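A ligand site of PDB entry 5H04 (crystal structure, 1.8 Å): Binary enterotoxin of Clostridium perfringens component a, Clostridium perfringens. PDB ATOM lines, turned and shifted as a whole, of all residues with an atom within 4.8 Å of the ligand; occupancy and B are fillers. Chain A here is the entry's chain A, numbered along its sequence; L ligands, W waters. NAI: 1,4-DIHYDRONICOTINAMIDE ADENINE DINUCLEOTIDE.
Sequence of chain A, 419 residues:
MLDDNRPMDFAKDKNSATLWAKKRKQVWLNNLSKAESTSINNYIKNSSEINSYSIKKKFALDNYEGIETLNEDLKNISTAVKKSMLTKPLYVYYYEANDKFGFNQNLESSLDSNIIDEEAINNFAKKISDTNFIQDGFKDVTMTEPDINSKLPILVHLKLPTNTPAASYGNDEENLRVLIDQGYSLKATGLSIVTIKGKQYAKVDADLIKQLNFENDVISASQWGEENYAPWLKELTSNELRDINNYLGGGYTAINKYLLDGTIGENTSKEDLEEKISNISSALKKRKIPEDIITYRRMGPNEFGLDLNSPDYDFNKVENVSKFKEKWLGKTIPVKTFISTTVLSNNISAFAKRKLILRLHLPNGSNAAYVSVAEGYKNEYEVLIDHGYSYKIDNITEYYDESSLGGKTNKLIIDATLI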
ATOM      1  N   TYR A 247     -27.274  24.873  -7.254  1.00  0.00           N
ATOM      2  CA  TYR A 247     -27.311  23.533  -6.675  1.00  0.00           C
ATOM      3  C   TYR A 247     -28.660  22.874  -6.923  1.00  0.00           C
ATOM      4  O   TYR A 247     -28.734  21.741  -7.413  1.00  0.00           O
ATOM      5  CB  TYR A 247     -26.994  23.636  -5.181  1.00  0.00           C
ATOM      6  CG  TYR A 247     -27.070  22.320  -4.431  1.00  0.00           C
ATOM      7  CD1 TYR A 247     -28.297  21.826  -3.981  1.00  0.00           C
ATOM      8  CD2 TYR A 247     -25.932  21.572  -4.172  1.00  0.00           C
ATOM      9  CE1 TYR A 247     -28.374  20.624  -3.300  1.00  0.00           C
ATOM     10  CE2 TYR A 247     -26.003  20.359  -3.489  1.00  0.00           C
ATOM     11  CZ  TYR A 247     -27.240  19.897  -3.050  1.00  0.00           C
ATOM     12  OH  TYR A 247     -27.346  18.700  -2.355  1.00  0.00           O
ATOM     13  N   LEU A 248     -29.746  23.583  -6.618  1.00  0.00           N
ATOM     14  CA  LEU A 248     -31.072  22.993  -6.677  1.00  0.00           C
ATOM     15  C   LEU A 248     -31.544  22.737  -8.096  1.00  0.00           C
ATOM     16  O   LEU A 248     -32.387  21.856  -8.300  1.00  0.00           O
ATOM     17  CB  LEU A 248     -32.073  23.876  -5.957  1.00  0.00           C
ATOM     18  CG  LEU A 248     -31.877  23.976  -4.444  1.00  0.00           C
ATOM     19  CD1 LEU A 248     -32.910  24.932  -3.868  1.00  0.00           C
ATOM     20  CD2 LEU A 248     -31.981  22.587  -3.779  1.00  0.00           C
ATOM     21  N   TYR A 252     -26.096  20.176  -8.107  1.00  0.00           N
ATOM     22  CA  TYR A 252     -25.799  19.219  -7.044  1.00  0.00           C
ATOM     23  C   TYR A 252     -24.902  18.096  -7.537  1.00  0.00           C
ATOM     24  O   TYR A 252     -24.059  17.591  -6.789  1.00  0.00           O
ATOM     25  CB  TYR A 252     -27.103  18.660  -6.482  1.00  0.00           C
ATOM     26  CG  TYR A 252     -27.952  17.977  -7.531  1.00  0.00           C
ATOM     27  CD1 TYR A 252     -27.739  16.645  -7.866  1.00  0.00           C
ATOM     28  CD2 TYR A 252     -28.947  18.676  -8.217  1.00  0.00           C
ATOM     29  CE1 TYR A 252     -28.467  16.031  -8.853  1.00  0.00           C
ATOM     30  CE2 TYR A 252     -29.699  18.057  -9.201  1.00  0.00           C
ATOM     31  CZ  TYR A 252     -29.451  16.733  -9.510  1.00  0.00           C
ATOM     32  OH  TYR A 252     -30.195  16.098 -10.478  1.00  0.00           O
ATOM     33  N   THR A 253     -25.080  17.677  -8.799  1.00  0.00           N
ATOM     34  CA  THR A 253     -24.303  16.547  -9.298  1.00  0.00           C
ATOM     35  C   THR A 253     -22.812  16.808  -9.166  1.00  0.00           C
ATOM     36  O   THR A 253     -22.077  16.011  -8.573  1.00  0.00           O
ATOM     37  CB  THR A 253     -24.666  16.257 -10.760  1.00  0.00           C
ATOM     38  OG1 THR A 253     -26.057  15.941 -10.858  1.00  0.00           O
ATOM     39  CG2 THR A 253     -23.832  15.094 -11.286  1.00  0.00           C
ATOM     40  N   ASN A 256     -21.782  17.869  -5.115  1.00  0.00           N
ATOM     41  CA  ASN A 256     -21.690  16.767  -4.153  1.00  0.00           C
ATOM     42  C   ASN A 256     -20.689  15.708  -4.598  1.00  0.00           C
ATOM     43  O   ASN A 256     -20.049  15.079  -3.751  1.00  0.00           O
ATOM     44  CB  ASN A 256     -23.073  16.148  -3.942  1.00  0.00           C
ATOM     45  CG  ASN A 256     -23.947  16.976  -3.027  1.00  0.00           C
ATOM     46  OD1 ASN A 256     -23.460  17.740  -2.195  1.00  0.00           O
ATOM     47  ND2 ASN A 256     -25.265  16.819  -3.170  1.00  0.00           N
ATOM     48  N   LEU A 260     -17.603  14.632  -2.157  1.00  0.00           N
ATOM     49  CA  LEU A 260     -17.441  13.221  -1.827  1.00  0.00           C
ATOM     50  C   LEU A 260     -15.999  12.753  -2.063  1.00  0.00           C
ATOM     51  O   LEU A 260     -15.400  12.103  -1.208  1.00  0.00           O
ATOM     52  CB  LEU A 260     -18.422  12.380  -2.649  1.00  0.00           C
ATOM     53  CG  LEU A 260     -18.390  10.869  -2.434  1.00  0.00           C
ATOM     54  CD1 LEU A 260     -18.575  10.536  -0.956  1.00  0.00           C
ATOM     55  CD2 LEU A 260     -19.448  10.151  -3.287  1.00  0.00           C
ATOM     56  N   TYR A 296     -36.898  13.592   5.162  1.00  0.00           N
ATOM     57  CA  TYR A 296     -36.788  12.344   4.404  1.00  0.00           C
ATOM     58  C   TYR A 296     -35.819  12.471   3.246  1.00  0.00           C
ATOM     59  O   TYR A 296     -35.601  13.565   2.704  1.00  0.00           O
ATOM     60  CB  TYR A 296     -38.149  11.894   3.870  1.00  0.00           C
ATOM     61  CG  TYR A 296     -39.166  11.661   4.959  1.00  0.00           C
ATOM     62  CD1 TYR A 296     -39.945  12.705   5.438  1.00  0.00           C
ATOM     63  CD2 TYR A 296     -39.358  10.392   5.488  1.00  0.00           C
ATOM     64  CE1 TYR A 296     -40.873  12.500   6.439  1.00  0.00           C
ATOM     65  CE2 TYR A 296     -40.291  10.171   6.498  1.00  0.00           C
ATOM     66  CZ  TYR A 296     -41.056  11.227   6.965  1.00  0.00           C
ATOM     67  OH  TYR A 296     -41.980  11.014   7.954  1.00  0.00           O
ATOM     68  N   ARG A 297     -35.247  11.335   2.839  1.00  0.00           N
ATOM     69  CA  ARG A 297     -34.399  11.346   1.656  1.00  0.00           C
ATOM     70  C   ARG A 297     -34.482   9.993   0.958  1.00  0.00           C
ATOM     71  O   ARG A 297     -34.335   8.949   1.599  1.00  0.00           O
ATOM     72  CB  ARG A 297     -32.931  11.676   2.016  1.00  0.00           C
ATOM     73  CG  ARG A 297     -32.000  11.588   0.812  1.00  0.00           C
ATOM     74  CD  ARG A 297     -30.539  11.996   1.137  1.00  0.00           C
ATOM     75  NE  ARG A 297     -29.655  11.561   0.058  1.00  0.00           N
ATOM     76  CZ  ARG A 297     -29.600  12.156  -1.130  1.00  0.00           C
ATOM     77  NH1 ARG A 297     -30.344  13.222  -1.391  1.00  0.00           N
ATOM     78  NH2 ARG A 297     -28.797  11.688  -2.086  1.00  0.00           N
ATOM     79  N   ARG A 298     -34.728  10.016  -0.351  1.00  0.00           N
ATOM     80  CA  ARG A 298     -34.594   8.808  -1.167  1.00  0.00           C
ATOM     81  C   ARG A 298     -33.125   8.663  -1.517  1.00  0.00           C
ATOM     82  O   ARG A 298     -32.567   9.479  -2.245  1.00  0.00           O
ATOM     83  CB  ARG A 298     -35.476   8.902  -2.411  1.00  0.00           C
ATOM     84  CG  ARG A 298     -36.959   8.999  -2.067  1.00  0.00           C
ATOM     85  CD  ARG A 298     -37.367   7.857  -1.134  1.00  0.00           C
ATOM     86  NE  ARG A 298     -38.693   8.078  -0.552  1.00  0.00           N
ATOM     87  CZ  ARG A 298     -39.725   7.261  -0.683  1.00  0.00           C
ATOM     88  NH1 ARG A 298     -39.596   6.138  -1.390  1.00  0.00           N
ATOM     89  NH2 ARG A 298     -40.882   7.557  -0.120  1.00  0.00           N
ATOM     90  N   MET A 299     -32.478   7.646  -0.940  1.00  0.00           N
ATOM     91  CA  MET A 299     -31.028   7.512  -0.999  1.00  0.00           C
ATOM     92  C   MET A 299     -30.641   6.531  -2.092  1.00  0.00           C
ATOM     93  O   MET A 299     -31.300   5.510  -2.303  1.00  0.00           O
ATOM     94  CB  MET A 299     -30.469   7.037   0.351  1.00  0.00           C
ATOM     95  CG  MET A 299     -30.745   7.992   1.509  1.00  0.00           C
ATOM     96  SD  MET A 299     -30.200   7.333   3.097  1.00  0.00           S
ATOM     97  CE  MET A 299     -28.494   7.846   3.123  1.00  0.00           C
ATOM     98  N   GLY A 300     -29.541   6.844  -2.780  1.00  0.00           N
ATOM     99  CA  GLY A 300     -28.973   5.930  -3.732  1.00  0.00           C
ATOM    100  C   GLY A 300     -28.071   4.935  -3.033  1.00  0.00           C
ATOM    101  O   GLY A 300     -27.626   5.155  -1.905  1.00  0.00           O
ATOM    102  N   PRO A 301     -27.756   3.818  -3.707  1.00  0.00           N
ATOM    103  CA  PRO A 301     -26.972   2.763  -3.037  1.00  0.00           C
ATOM    104  C   PRO A 301     -25.547   3.151  -2.720  1.00  0.00           C
ATOM    105  O   PRO A 301     -24.939   2.559  -1.811  1.00  0.00           O
ATOM    106  CB  PRO A 301     -27.032   1.603  -4.032  1.00  0.00           C
ATOM    107  CG  PRO A 301     -27.218   2.286  -5.356  1.00  0.00           C
ATOM    108  CD  PRO A 301     -28.149   3.422  -5.063  1.00  0.00           C
ATOM    109  N   ASN A 302     -24.957   4.106  -3.448  1.00  0.00           N
ATOM    110  CA  ASN A 302     -23.601   4.553  -3.147  1.00  0.00           C
ATOM    111  C   ASN A 302     -23.495   5.148  -1.758  1.00  0.00           C
ATOM    112  O   ASN A 302     -22.403   5.139  -1.158  1.00  0.00           O
ATOM    113  CB  ASN A 302     -23.129   5.596  -4.165  1.00  0.00           C
ATOM    114  CG  ASN A 302     -22.988   5.051  -5.578  1.00  0.00           C
ATOM    115  OD1 ASN A 302     -22.805   5.823  -6.514  1.00  0.00           O
ATOM    116  ND2 ASN A 302     -23.088   3.729  -5.747  1.00  0.00           N
ATOM    117  N   GLU A 303     -24.579   5.705  -1.215  1.00  0.00           N
ATOM    118  CA  GLU A 303     -24.508   6.256   0.128  1.00  0.00           C
ATOM    119  C   GLU A 303     -24.270   5.185   1.180  1.00  0.00           C
ATOM    120  O   GLU A 303     -23.961   5.518   2.327  1.00  0.00           O
ATOM    121  CB  GLU A 303     -25.785   7.057   0.418  1.00  0.00           C
ATOM    122  CG  GLU A 303     -25.904   8.261  -0.531  1.00  0.00           C
ATOM    123  CD  GLU A 303     -27.288   8.880  -0.602  1.00  0.00           C
ATOM    124  OE1 GLU A 303     -27.814   9.377   0.424  1.00  0.00           O
ATOM    125  OE2 GLU A 303     -27.850   8.909  -1.716  1.00  0.00           O
ATOM    126  N   VAL A 335     -20.971  12.211   6.692  1.00  0.00           N
ATOM    127  CA  VAL A 335     -21.583  12.649   5.452  1.00  0.00           C
ATOM    128  C   VAL A 335     -20.823  13.863   4.949  1.00  0.00           C
ATOM    129  O   VAL A 335     -20.963  14.970   5.494  1.00  0.00           O
ATOM    130  CB  VAL A 335     -23.072  12.983   5.631  1.00  0.00           C
ATOM    131  CG1 VAL A 335     -23.679  13.397   4.299  1.00  0.00           C
ATOM    132  CG2 VAL A 335     -23.839  11.781   6.206  1.00  0.00           C
ATOM    133  N   LYS A 336     -20.019  13.670   3.905  1.00  0.00           N
ATOM    134  CA  LYS A 336     -19.190  14.740   3.361  1.00  0.00           C
ATOM    135  C   LYS A 336     -19.977  15.690   2.472  1.00  0.00           C
ATOM    136  O   LYS A 336     -19.536  16.829   2.245  1.00  0.00           O
ATOM    137  CB  LYS A 336     -18.027  14.158   2.551  1.00  0.00           C
ATOM    138  CG  LYS A 336     -17.223  13.127   3.322  1.00  0.00           C
ATOM    139  CD  LYS A 336     -16.105  12.530   2.469  1.00  0.00           C
ATOM    140  CE  LYS A 336     -15.007  13.548   2.203  1.00  0.00           C
ATOM    141  NZ  LYS A 336     -13.861  12.921   1.487  1.00  0.00           N
ATOM    142  N   THR A 337     -21.137  15.267   1.989  1.00  0.00           N
ATOM    143  CA  THR A 337     -21.911  16.029   1.025  1.00  0.00           C
ATOM    144  C   THR A 337     -22.902  16.944   1.723  1.00  0.00           C
ATOM    145  O   THR A 337     -23.199  16.801   2.918  1.00  0.00           O
ATOM    146  CB  THR A 337     -22.671  15.063   0.106  1.00  0.00           C
ATOM    147  OG1 THR A 337     -23.336  14.076   0.904  1.00  0.00           O
ATOM    148  CG2 THR A 337     -21.724  14.370  -0.854  1.00  0.00           C
ATOM    149  N   SER A 340     -29.541  16.715   0.582  1.00  0.00           N
ATOM    150  CA  SER A 340     -30.864  17.106   0.093  1.00  0.00           C
ATOM    151  C   SER A 340     -31.929  16.189   0.715  1.00  0.00           C
ATOM    152  O   SER A 340     -31.929  14.977   0.474  1.00  0.00           O
ATOM    153  CB  SER A 340     -30.919  17.037  -1.425  1.00  0.00           C
ATOM    154  OG  SER A 340     -30.201  18.121  -2.014  1.00  0.00           O
ATOM    155  N   THR A 341     -32.827  16.776   1.514  1.00  0.00           N
ATOM    156  CA  THR A 341     -33.943  16.068   2.134  1.00  0.00           C
ATOM    157  C   THR A 341     -35.241  16.785   1.779  1.00  0.00           C
ATOM    158  O   THR A 341     -35.241  17.860   1.191  1.00  0.00           O
ATOM    159  CB  THR A 341     -33.804  15.964   3.667  1.00  0.00           C
ATOM    160  OG1 THR A 341     -34.065  17.251   4.251  1.00  0.00           O
ATOM    161  CG2 THR A 341     -32.408  15.507   4.049  1.00  0.00           C
ATOM    162  N   THR A 342     -36.360  16.146   2.129  1.00  0.00           N
ATOM    163  CA  THR A 342     -37.670  16.736   1.932  1.00  0.00           C
ATOM    164  C   THR A 342     -38.483  16.485   3.191  1.00  0.00           C
ATOM    165  O   THR A 342     -38.336  15.440   3.832  1.00  0.00           O
ATOM    166  CB  THR A 342     -38.387  16.164   0.694  1.00  0.00           C
ATOM    167  OG1 THR A 342     -39.752  16.623   0.667  1.00  0.00           O
ATOM    168  CG2 THR A 342     -38.400  14.665   0.741  1.00  0.00           C
ATOM    169  N   ILE A 348     -40.783  10.080  -4.814  1.00  0.00           N
ATOM    170  CA  ILE A 348     -40.535  11.117  -5.806  1.00  0.00           C
ATOM    171  C   ILE A 348     -40.267  10.464  -7.161  1.00  0.00           C
ATOM    172  O   ILE A 348     -39.412   9.574  -7.260  1.00  0.00           O
ATOM    173  CB  ILE A 348     -39.347  12.009  -5.399  1.00  0.00           C
ATOM    174  CG1 ILE A 348     -39.669  12.789  -4.116  1.00  0.00           C
ATOM    175  CG2 ILE A 348     -38.946  12.939  -6.546  1.00  0.00           C
ATOM    176  CD1 ILE A 348     -38.473  13.493  -3.507  1.00  0.00           C
ATOM    177  N   PHE A 351     -36.888   9.676  -8.378  1.00  0.00           N
ATOM    178  CA  PHE A 351     -36.161   8.756  -7.507  1.00  0.00           C
ATOM    179  C   PHE A 351     -37.016   7.547  -7.130  1.00  0.00           C
ATOM    180  O   PHE A 351     -36.761   6.909  -6.103  1.00  0.00           O
ATOM    181  CB  PHE A 351     -35.700   9.470  -6.236  1.00  0.00           C
ATOM    182  CG  PHE A 351     -35.090  10.824  -6.477  1.00  0.00           C
ATOM    183  CD1 PHE A 351     -33.944  10.961  -7.226  1.00  0.00           C
ATOM    184  CD2 PHE A 351     -35.669  11.959  -5.941  1.00  0.00           C
ATOM    185  CE1 PHE A 351     -33.379  12.213  -7.454  1.00  0.00           C
ATOM    186  CE2 PHE A 351     -35.112  13.216  -6.166  1.00  0.00           C
ATOM    187  CZ  PHE A 351     -33.980  13.328  -6.921  1.00  0.00           C
ATOM    188  N   ARG A 354     -35.263   4.157  -6.038  1.00  0.00           N
ATOM    189  CA  ARG A 354     -34.300   4.046  -4.954  1.00  0.00           C
ATOM    190  C   ARG A 354     -34.905   3.245  -3.809  1.00  0.00           C
ATOM    191  O   ARG A 354     -36.084   3.408  -3.478  1.00  0.00           O
ATOM    192  CB  ARG A 354     -33.864   5.433  -4.467  1.00  0.00           C
ATOM    193  CG  ARG A 354     -33.149   6.249  -5.543  1.00  0.00           C
ATOM    194  CD  ARG A 354     -32.481   7.477  -4.993  1.00  0.00           C
ATOM    195  NE  ARG A 354     -31.855   8.237  -6.079  1.00  0.00           N
ATOM    196  CZ  ARG A 354     -31.324   9.443  -5.940  1.00  0.00           C
ATOM    197  NH1 ARG A 354     -31.353  10.061  -4.763  1.00  0.00           N
ATOM    198  NH2 ARG A 354     -30.782  10.053  -6.992  1.00  0.00           N
ATOM    199  N   GLU A 380     -40.334  20.852  -4.332  1.00  0.00           N
ATOM    200  CA  GLU A 380     -40.247  19.535  -3.721  1.00  0.00           C
ATOM    201  C   GLU A 380     -40.115  19.595  -2.203  1.00  0.00           C
ATOM    202  O   GLU A 380     -39.697  18.605  -1.588  1.00  0.00           O
ATOM    203  CB  GLU A 380     -39.086  18.757  -4.344  1.00  0.00           C
ATOM    204  CG  GLU A 380     -39.264  18.436  -5.831  1.00  0.00           C
ATOM    205  CD  GLU A 380     -40.139  17.217  -6.098  1.00  0.00           C
ATOM    206  OE1 GLU A 380     -40.984  16.864  -5.232  1.00  0.00           O
ATOM    207  OE2 GLU A 380     -39.984  16.606  -7.174  1.00  0.00           O
ATOM    208  N   GLU A 382     -38.176  21.046   0.129  1.00  0.00           N
ATOM    209  CA  GLU A 382     -36.828  20.569   0.423  1.00  0.00           C
ATOM    210  C   GLU A 382     -36.221  21.266   1.635  1.00  0.00           C
ATOM    211  O   GLU A 382     -36.324  22.487   1.790  1.00  0.00           O
ATOM    212  CB  GLU A 382     -35.891  20.771  -0.767  1.00  0.00           C
ATOM    213  CG  GLU A 382     -36.334  20.109  -2.062  1.00  0.00           C
ATOM    214  CD  GLU A 382     -35.267  20.248  -3.143  1.00  0.00           C
ATOM    215  OE1 GLU A 382     -34.073  20.043  -2.837  1.00  0.00           O
ATOM    216  OE2 GLU A 382     -35.652  20.574  -4.290  1.00  0.00           O
HETATM  217  PA  NAI L   1     -27.362  13.958  -4.685  1.00  0.00           P
HETATM  218  O1A NAI L   1     -26.134  14.812  -5.128  1.00  0.00           O
HETATM  219  O2A NAI L   1     -27.481  13.874  -3.157  1.00  0.00           O
HETATM  220  O5B NAI L   1     -27.215  12.439  -5.240  1.00  0.00           O
HETATM  221  C5B NAI L   1     -27.006  12.127  -6.607  1.00  0.00           C
HETATM  222  C4B NAI L   1     -26.264  10.763  -6.633  1.00  0.00           C
HETATM  223  O4B NAI L   1     -24.989  10.878  -5.747  1.00  0.00           O
HETATM  224  C3B NAI L   1     -26.969   9.830  -6.127  1.00  0.00           C
HETATM  225  O3B NAI L   1     -26.778   8.565  -6.820  1.00  0.00           O
HETATM  226  C2B NAI L   1     -26.432   9.612  -4.581  1.00  0.00           C
HETATM  227  O2B NAI L   1     -26.769   8.272  -4.148  1.00  0.00           O
HETATM  228  C1B NAI L   1     -25.175   9.848  -4.606  1.00  0.00           C
HETATM  229  N9A NAI L   1     -24.732  10.497  -3.367  1.00  0.00           N
HETATM  230  C8A NAI L   1     -25.195  11.648  -2.815  1.00  0.00           C
HETATM  231  N7A NAI L   1     -24.476  11.841  -1.651  1.00  0.00           N
HETATM  232  C5A NAI L   1     -23.579  10.795  -1.521  1.00  0.00           C
HETATM  233  C6A NAI L   1     -22.648  10.521  -0.550  1.00  0.00           C
HETATM  234  N6A NAI L   1     -22.252  11.171   0.651  1.00  0.00           N
HETATM  235  N1A NAI L   1     -21.888   9.411  -0.650  1.00  0.00           N
HETATM  236  C2A NAI L   1     -22.051   8.562  -1.719  1.00  0.00           C
HETATM  237  N3A NAI L   1     -22.970   8.840  -2.698  1.00  0.00           N
HETATM  238  C4A NAI L   1     -23.735   9.958  -2.587  1.00  0.00           C
HETATM  239  O3  NAI L   1     -28.694  14.554  -5.334  1.00  0.00           O
HETATM  240  PN  NAI L   1     -30.097  13.785  -5.511  1.00  0.00           P
HETATM  241  O1N NAI L   1     -30.494  13.023  -4.312  1.00  0.00           O
HETATM  242  O2N NAI L   1     -30.083  12.809  -6.700  1.00  0.00           O
HETATM  243  O5D NAI L   1     -31.172  14.961  -5.707  1.00  0.00           O
HETATM  244  C5D NAI L   1     -31.181  15.679  -6.883  1.00  0.00           C
HETATM  245  C4D NAI L   1     -32.088  16.807  -6.761  1.00  0.00           C
HETATM  246  O4D NAI L   1     -33.263  16.414  -6.267  1.00  0.00           O
HETATM  247  C3D NAI L   1     -31.483  17.957  -5.738  1.00  0.00           C
HETATM  248  O3D NAI L   1     -31.871  19.302  -6.285  1.00  0.00           O
HETATM  249  C2D NAI L   1     -32.020  17.739  -4.648  1.00  0.00           C
HETATM  250  O2D NAI L   1     -32.085  18.926  -3.760  1.00  0.00           O
HETATM  251  C1D NAI L   1     -33.514  17.246  -5.061  1.00  0.00           C
HETATM  252  N1N NAI L   1     -34.112  16.543  -4.119  1.00  0.00           N
HETATM  253  C2N NAI L   1     -33.599  15.283  -3.671  1.00  0.00           C
HETATM  254  C3N NAI L   1     -34.381  14.485  -2.617  1.00  0.00           C
HETATM  255  C7N NAI L   1     -34.103  13.052  -2.364  1.00  0.00           C
HETATM  256  O7N NAI L   1     -34.894  12.434  -1.619  1.00  0.00           O
HETATM  257  N7N NAI L   1     -32.989  12.401  -2.926  1.00  0.00           N
HETATM  258  C4N NAI L   1     -35.446  15.167  -1.761  1.00  0.00           C
HETATM  259  C5N NAI L   1     -36.140  16.287  -2.537  1.00  0.00           C
HETATM  260  C6N NAI L   1     -35.330  17.069  -3.549  1.00  0.00           C
HETATM  261  O   HOH W   1     -27.622  14.894  -0.698  1.00  0.00           O
HETATM  262  O   HOH W   2     -33.086  19.209  -0.484  1.00  0.00           O
HETATM  263  O   HOH W   3     -24.390   7.668  -7.611  1.00  0.00           O
HETATM  264  O   HOH W   4     -21.617   8.343  -5.363  1.00  0.00           O
HETATM  265  O   HOH W   5     -23.750  14.260  -6.688  1.00  0.00           O
HETATM  266  O   HOH W   6     -20.067   7.828   0.797  1.00  0.00           O
HETATM  267  O   HOH W   7     -24.362  12.349  -8.711  1.00  0.00           O
HETATM  268  O   HOH W   8     -22.604  12.599  -5.216  1.00  0.00           O
HETATM  269  O   HOH W   9     -26.076   5.855  -5.414  1.00  0.00           O
HETATM  270  O   HOH W  10     -25.978  13.076   0.541  1.00  0.00           O
HETATM  271  O   HOH W  11     -20.223  11.063   2.380  1.00  0.00           O
HETATM  272  O   HOH W  12     -35.148  17.034  -7.919  1.00  0.00           O
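The backbone carbonyl oxygen (O) of Ser 340 sits at hydrogen-bond distance from the guanidinium group (NH1) of Arg 297, 3.0 Å away. OH of Tyr 247 sits at hydrogen-bond distance from OG of Ser 340 (2.9 Å). The backbone carbonyl oxygen of Arg 298 lies within hydrogen-bond range of the guanidinium group of Arg 354 (2.9 Å). The side-chain carboxylate of Glu 303 is in salt-bridge range of the guanidinium group of Arg 297, at 2.9 Å. The side-chain carboxylate of Glu 303 lies within hydrogen-bond range of the backbone NH of Gly 300, at 2.9 Å. The side-chain amino group (NZ) of Lys 336 lies within hydrogen-bond range of the backbone carbonyl oxygen (O) of Leu 260, at 3.2 Å. OG1 of Thr 342 lies within hydrogen-bond range of O of Glu 380 (3.0 Å). O of Thr 342 is in hydrogen-bond range of N of Tyr 296.
CZ of Tyr 252 touches C5D of the ligand, 3.3 Å away. Leu 260 touches the ligand. O of Asn 302 touches C2A of the ligand (3.5 Å). Thr 341 touches the ligand. CG2 of Thr 342 touches C4N of the ligand (3.9 Å). CD1 of Ile 348 touches C5N of the ligand, 3.8 Å away. CZ of Phe 351 touches O4D of the ligand, at 3.2 Å. Hydrophobic or aromatic side chains that line the ligand: Leu 248, Tyr 252, Leu 260, Ile 348 and Phe 351. Of the 25 residues printed, 17 come within 4 Å of the ligand. The nearest printed residue that does not touch the ligand is Tyr 247 (4.1 Å).
The side-chain carboxylate (OE1) of Glu 382 sits at hydrogen-bond distance from an oxygen (O2D) of the ligand (2.5 Å). O2D of the ligand sits at hydrogen-bond distance from OG of Ser 340 (2.7 Å). N of Arg 298 sits at hydrogen-bond distance from O7N of the ligand, at 2.7 Å. O of Arg 298 sits at hydrogen-bond distance from N7N of the ligand. An oxygen (O2B) of the ligand lies within hydrogen-bond range of the side-chain carboxylate (OE2) of Glu 303 (2.7 Å). The guanidinium group (NH2) of Arg 297 is in salt-bridge range of an oxygen (O2A) of the ligand, 2.8 Å away. The guanidinium group of Arg 354 lies within salt-bridge range of an oxygen (O2N) of the ligand (2.9 Å). ND2 of Asn 256 lies within hydrogen-bond range of O1A of the ligand (2.9 Å). The side-chain hydroxyl of Thr 337 is in hydrogen-bond range of a nitrogen (N6A) of the ligand (3.1 Å). The backbone NH (N) of Gly 300 lies close to an oxygen (O2B) of the ligand, at 3.4 Å. An oxygen (O3D) of the ligand is in hydrogen-bond range of the backbone carbonyl oxygen (O) of Leu 248 (3.3 Å).
Water W1 lies within hydrogen-bond range of an oxygen (O2A) of the ligand (2.7 Å), the backbone NH (N) of Ser 340 (2.9 Å) and the guanidinium group (NH1) of Arg 297 (3.3 Å). Water W3 lies within hydrogen-bond range of the side-chain amide oxygen of Asn 302 and an oxygen (O3B) of the ligand. Water W9 lies within hydrogen-bond range of an oxygen (O2B) of the ligand (2.8 Å) and the backbone NH of Asn 302 (2.9 Å). Water W10 lies within hydrogen-bond range of the side-chain hydroxyl of Thr 337 (2.8 Å) and a nitrogen (N7A) of the ligand (2.9 Å). Water W4 bridges OD1 of Asn 302 and N3A of the ligand. Water W2 lies within hydrogen-bond range of OE1 of Glu 382, O of Thr 341, O2D of the ligand and OG of Ser 340.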
